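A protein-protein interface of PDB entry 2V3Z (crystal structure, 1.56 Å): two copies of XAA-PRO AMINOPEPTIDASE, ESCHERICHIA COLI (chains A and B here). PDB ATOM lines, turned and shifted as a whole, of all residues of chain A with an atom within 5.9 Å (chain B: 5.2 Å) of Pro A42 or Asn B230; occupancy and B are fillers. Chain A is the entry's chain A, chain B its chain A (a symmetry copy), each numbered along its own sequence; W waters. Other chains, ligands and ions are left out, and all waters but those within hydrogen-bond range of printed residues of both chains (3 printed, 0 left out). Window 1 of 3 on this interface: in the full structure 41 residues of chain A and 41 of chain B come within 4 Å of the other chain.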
ATOM      1  N   GLU A  40      -1.528  12.290 -12.004  1.00  0.00           N
ATOM      2  CA  GLU A  40      -2.971  12.433 -11.973  1.00  0.00           C
ATOM      3  C   GLU A  40      -3.573  12.181 -13.355  1.00  0.00           C
ATOM      4  O   GLU A  40      -2.912  12.341 -14.385  1.00  0.00           O
ATOM      5  CB  GLU A  40      -3.330  13.842 -11.486  1.00  0.00           C
ATOM      6  CG  GLU A  40      -2.823  14.153 -10.066  1.00  0.00           C
ATOM      7  CD  GLU A  40      -2.955  15.626  -9.690  1.00  0.00           C
ATOM      8  OE1 GLU A  40      -3.498  16.403 -10.501  1.00  0.00           O
ATOM      9  OE2 GLU A  40      -2.506  16.000  -8.592  1.00  0.00           O
ATOM     10  N   TYR A  41      -4.826  11.759 -13.370  1.00  0.00           N
ATOM     11  CA  TYR A  41      -5.560  11.677 -14.597  1.00  0.00           C
ATOM     12  C   TYR A  41      -5.782  13.094 -15.122  1.00  0.00           C
ATOM     13  O   TYR A  41      -5.825  14.040 -14.321  1.00  0.00           O
ATOM     14  CB  TYR A  41      -6.927  11.019 -14.336  1.00  0.00           C
ATOM     15  CG  TYR A  41      -6.909   9.499 -14.219  1.00  0.00           C
ATOM     16  CD1 TYR A  41      -6.771   8.703 -15.340  1.00  0.00           C
ATOM     17  CD2 TYR A  41      -7.066   8.873 -12.984  1.00  0.00           C
ATOM     18  CE1 TYR A  41      -6.773   7.331 -15.245  1.00  0.00           C
ATOM     19  CE2 TYR A  41      -7.064   7.486 -12.880  1.00  0.00           C
ATOM     20  CZ  TYR A  41      -6.936   6.728 -13.998  1.00  0.00           C
ATOM     21  OH  TYR A  41      -6.951   5.347 -13.850  1.00  0.00           O
ATOM     22  N   PRO A  42      -6.019  13.222 -16.429  1.00  0.00           N
ATOM     23  CA  PRO A  42      -6.403  14.528 -16.969  1.00  0.00           C
ATOM     24  C   PRO A  42      -7.673  15.004 -16.266  1.00  0.00           C
ATOM     25  O   PRO A  42      -8.619  14.234 -16.074  1.00  0.00           O
ATOM     26  CB  PRO A  42      -6.718  14.256 -18.432  1.00  0.00           C
ATOM     27  CG  PRO A  42      -6.227  12.893 -18.725  1.00  0.00           C
ATOM     28  CD  PRO A  42      -6.029  12.156 -17.434  1.00  0.00           C
ATOM     29  N   TYR A  43      -7.700  16.269 -15.907  1.00  0.00           N
ATOM     30  CA  TYR A  43      -8.764  16.805 -15.071  1.00  0.00           C
ATOM     31  C   TYR A  43     -10.070  16.816 -15.834  1.00  0.00           C
ATOM     32  O   TYR A  43     -10.122  17.216 -17.005  1.00  0.00           O
ATOM     33  CB  TYR A  43      -8.400  18.216 -14.624  1.00  0.00           C
ATOM     34  CG  TYR A  43      -9.377  18.802 -13.644  1.00  0.00           C
ATOM     35  CD1 TYR A  43      -9.516  18.254 -12.370  1.00  0.00           C
ATOM     36  CD2 TYR A  43     -10.177  19.887 -13.979  1.00  0.00           C
ATOM     37  CE1 TYR A  43     -10.455  18.760 -11.462  1.00  0.00           C
ATOM     38  CE2 TYR A  43     -11.091  20.386 -13.101  1.00  0.00           C
ATOM     39  CZ  TYR A  43     -11.227  19.845 -11.835  1.00  0.00           C
ATOM     40  OH  TYR A  43     -12.142  20.375 -10.922  1.00  0.00           O
ATOM     41  N   ARG A  44     -11.132  16.410 -15.147  1.00  0.00           N
ATOM     42  CA  ARG A  44     -12.499  16.490 -15.666  1.00  0.00           C
ATOM     43  C   ARG A  44     -13.324  17.256 -14.633  1.00  0.00           C
ATOM     44  O   ARG A  44     -13.552  16.783 -13.524  1.00  0.00           O
ATOM     45  CB  ARG A  44     -13.072  15.097 -15.931  1.00  0.00           C
ATOM     46  CG  ARG A  44     -14.563  15.075 -16.328  1.00  0.00           C
ATOM     47  CD  ARG A  44     -14.945  16.094 -17.423  1.00  0.00           C
ATOM     48  NE  ARG A  44     -16.112  15.536 -18.121  1.00  0.00           N
ATOM     49  CZ  ARG A  44     -17.341  15.441 -17.624  1.00  0.00           C
ATOM     50  NH1 ARG A  44     -17.665  15.980 -16.455  1.00  0.00           N
ATOM     51  NH2 ARG A  44     -18.302  14.810 -18.305  1.00  0.00           N
ATOM     52  N   TYR A 226     -10.720  14.342 -25.537  1.00  0.00           N
ATOM     53  CA  TYR A 226     -10.978  13.185 -24.708  1.00  0.00           C
ATOM     54  C   TYR A 226     -12.294  12.533 -25.130  1.00  0.00           C
ATOM     55  O   TYR A 226     -13.245  13.223 -25.538  1.00  0.00           O
ATOM     56  CB  TYR A 226     -11.078  13.573 -23.224  1.00  0.00           C
ATOM     57  CG  TYR A 226      -9.844  14.305 -22.689  1.00  0.00           C
ATOM     58  CD1 TYR A 226      -8.637  13.685 -22.614  1.00  0.00           C
ATOM     59  CD2 TYR A 226      -9.930  15.627 -22.335  1.00  0.00           C
ATOM     60  CE1 TYR A 226      -7.509  14.393 -22.160  1.00  0.00           C
ATOM     61  CE2 TYR A 226      -8.830  16.319 -21.886  1.00  0.00           C
ATOM     62  CZ  TYR A 226      -7.632  15.674 -21.803  1.00  0.00           C
ATOM     63  OH  TYR A 226      -6.492  16.343 -21.364  1.00  0.00           O
ATOM     64  N   TYR B  41     -12.635   6.500 -15.082  1.00  0.00           N
ATOM     65  CA  TYR B  41     -11.442   6.556 -15.872  1.00  0.00           C
ATOM     66  C   TYR B  41     -11.022   5.127 -16.215  1.00  0.00           C
ATOM     67  O   TYR B  41     -11.335   4.201 -15.452  1.00  0.00           O
ATOM     68  CB  TYR B  41     -10.319   7.227 -15.061  1.00  0.00           C
ATOM     69  CG  TYR B  41     -10.378   8.750 -14.999  1.00  0.00           C
ATOM     70  CD1 TYR B  41     -10.012   9.517 -16.088  1.00  0.00           C
ATOM     71  CD2 TYR B  41     -10.768   9.405 -13.834  1.00  0.00           C
ATOM     72  CE1 TYR B  41     -10.044  10.891 -16.035  1.00  0.00           C
ATOM     73  CE2 TYR B  41     -10.807  10.794 -13.775  1.00  0.00           C
ATOM     74  CZ  TYR B  41     -10.433  11.525 -14.856  1.00  0.00           C
ATOM     75  OH  TYR B  41     -10.477  12.909 -14.749  1.00  0.00           O
ATOM     76  N   SER B 228       2.056   7.345 -20.130  1.00  0.00           N
ATOM     77  CA  SER B 228       2.497   7.165 -18.738  1.00  0.00           C
ATOM     78  C   SER B 228       2.257   8.398 -17.880  1.00  0.00           C
ATOM     79  O   SER B 228       2.344   8.331 -16.638  1.00  0.00           O
ATOM     80  CB  SER B 228       3.965   6.751 -18.700  1.00  0.00           C
ATOM     81  OG  SER B 228       4.781   7.670 -19.385  1.00  0.00           O
ATOM     82  N   TYR B 229       1.964   9.527 -18.513  1.00  0.00           N
ATOM     83  CA  TYR B 229       1.654  10.789 -17.847  1.00  0.00           C
ATOM     84  C   TYR B 229       0.993  11.674 -18.879  1.00  0.00           C
ATOM     85  O   TYR B 229       1.074  11.409 -20.066  1.00  0.00           O
ATOM     86  CB  TYR B 229       2.892  11.465 -17.261  1.00  0.00           C
ATOM     87  CG  TYR B 229       3.990  11.688 -18.240  1.00  0.00           C
ATOM     88  CD1 TYR B 229       4.895  10.678 -18.542  1.00  0.00           C
ATOM     89  CD2 TYR B 229       4.139  12.904 -18.935  1.00  0.00           C
ATOM     90  CE1 TYR B 229       5.904  10.844 -19.471  1.00  0.00           C
ATOM     91  CE2 TYR B 229       5.152  13.071 -19.851  1.00  0.00           C
ATOM     92  CZ  TYR B 229       6.005  12.038 -20.155  1.00  0.00           C
ATOM     93  OH  TYR B 229       7.024  12.209 -21.067  1.00  0.00           O
ATOM     94  N   ASN B 230       0.374  12.750 -18.433  1.00  0.00           N
ATOM     95  CA  ASN B 230      -0.332  13.635 -19.353  1.00  0.00           C
ATOM     96  C   ASN B 230       0.664  14.395 -20.239  1.00  0.00           C
ATOM     97  O   ASN B 230       1.558  15.074 -19.744  1.00  0.00           O
ATOM     98  CB  ASN B 230      -1.243  14.594 -18.596  1.00  0.00           C
ATOM     99  CG  ASN B 230      -2.280  13.857 -17.762  1.00  0.00           C
ATOM    100  OD1 ASN B 230      -2.805  12.826 -18.191  1.00  0.00           O
ATOM    101  ND2 ASN B 230      -2.540  14.354 -16.575  1.00  0.00           N
ATOM    102  N   THR B 231       0.471  14.271 -21.550  1.00  0.00           N
ATOM    103  CA  THR B 231       1.364  14.803 -22.585  1.00  0.00           C
ATOM    104  C   THR B 231       1.406  16.310 -22.524  1.00  0.00           C
ATOM    105  O   THR B 231       0.371  16.956 -22.422  1.00  0.00           O
ATOM    106  CB  THR B 231       0.836  14.359 -23.937  1.00  0.00           C
ATOM    107  OG1 THR B 231       0.958  12.920 -23.977  1.00  0.00           O
ATOM    108  CG2 THR B 231       1.634  14.969 -25.092  1.00  0.00           C
ATOM    109  N   ILE B 232       2.638  16.841 -22.564  1.00  0.00           N
ATOM    110  CA  ILE B 232       2.925  18.279 -22.561  1.00  0.00           C
ATOM    111  C   ILE B 232       3.329  18.715 -23.973  1.00  0.00           C
ATOM    112  O   ILE B 232       4.267  18.146 -24.546  1.00  0.00           O
ATOM    113  CB  ILE B 232       4.111  18.526 -21.592  1.00  0.00           C
ATOM    114  CG1 ILE B 232       3.680  18.234 -20.151  1.00  0.00           C
ATOM    115  CG2 ILE B 232       4.715  19.916 -21.733  1.00  0.00           C
ATOM    116  CD1 ILE B 232       4.815  17.757 -19.219  1.00  0.00           C
ATOM    117  N   THR B 245      -0.103  21.270 -19.761  1.00  0.00           N
ATOM    118  CA  THR B 245      -0.915  20.271 -20.432  1.00  0.00           C
ATOM    119  C   THR B 245      -2.190  20.822 -21.064  1.00  0.00           C
ATOM    120  O   THR B 245      -2.961  20.029 -21.640  1.00  0.00           O
ATOM    121  CB  THR B 245      -1.265  19.104 -19.497  1.00  0.00           C
ATOM    122  OG1 THR B 245      -2.033  19.599 -18.390  1.00  0.00           O
ATOM    123  CG2 THR B 245       0.011  18.407 -19.006  1.00  0.00           C
ATOM    124  N   ASP B 260       6.882  16.905 -24.175  1.00  0.00           N
ATOM    125  CA  ASP B 260       7.296  15.942 -23.140  1.00  0.00           C
ATOM    126  C   ASP B 260       6.179  14.909 -23.095  1.00  0.00           C
ATOM    127  O   ASP B 260       5.065  15.199 -22.717  1.00  0.00           O
ATOM    128  CB  ASP B 260       7.490  16.688 -21.814  1.00  0.00           C
ATOM    129  CG  ASP B 260       8.217  15.890 -20.752  1.00  0.00           C
ATOM    130  OD1 ASP B 260       8.277  14.656 -20.890  1.00  0.00           O
ATOM    131  OD2 ASP B 260       8.749  16.545 -19.816  1.00  0.00           O
HETATM  132  O   HOH W   1     -10.279  14.753 -12.683  1.00  0.00           O
HETATM  133  O   HOH W   2      -2.031  10.174 -16.784  1.00  0.00           O
HETATM  134  O   HOH W   3      -0.165  12.551 -15.490  1.00  0.00           O
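The backbone carbonyl oxygen (O) of Pro A42 sits at hydrogen-bond distance from the side-chain hydroxyl (OH) of Tyr B41 (2.6 Å). The backbone carbonyl oxygen (O) of Glu A40 is in hydrogen-bond range of the side-chain amide nitrogen (ND2) of Asn B230 (3.0 Å).
Among the printed residues, merely in contact across the chains: Pro A42 with Asn B230, Tyr A41 with Tyr B41, Arg A44 with Tyr B41 and Tyr A41 with Asn B230.
Printed residues of chain B within 4 Å of Tyr A41: Tyr B41 and Asn B230. Pro A42 touches two residues of chain B. Of the printed residues of chain B, Arg A44 touches Tyr B41 (3.6 Å). Of the printed residues of chain A, Tyr B41 touches Tyr A41, Pro A42 and Arg A44. Of the printed residues of chain A, Asn B230 touches Glu A40, Tyr A41 and Pro A42. Thr B231 touches none of the printed residues of chain A. Thr B245 touches none of the printed residues of chain A. The nearest printed residue of chain B that does not touch Pro A42 is Thr B245 (6.8 Å). The nearest printed residue of chain A that does not touch Asn B230 is Tyr A43 (5.5 Å). The nearest printed residue of chain B that does not touch Arg A44 is Asn B230 (8.9 Å).
Of the 8 printed residues of chain B, 2 touch a printed residue of chain A. Hydrophobic or aromatic side chains of chain B that line the printed part of chain A: Tyr B41. Along chain B the printed residues that touch a printed residue of chain A span positions 41 to 230. Of the 6 printed residues of chain A, 4 touch a printed residue of chain B. Hydrophobic or aromatic side chains of chain A that line the printed part of chain B: Tyr A41 and Pro A42. Among the printed residues, no Asp or Glu carboxylate lies within 4 Å of a Lys or Arg side-chain nitrogen of the other chain.
Tyr B41 touches its own counterpart, Tyr A41. Position printed for both chains: 41. Of the 6 pairs that touch across the chains among the printed residues, 1 has its exchanged pair printed and touching as well.
Water W1 bridges OH of Tyr B41 (2.8 Å) and N of Arg A44 (3.1 Å). Water W3 bridges the backbone carbonyl oxygen (O) of Glu A40 (3.0 Å) and the backbone NH (N) of Asn B230 (3.0 Å). Water W2 lies within hydrogen-bond range of OD1 of Asn B230 and O of Glu A40.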
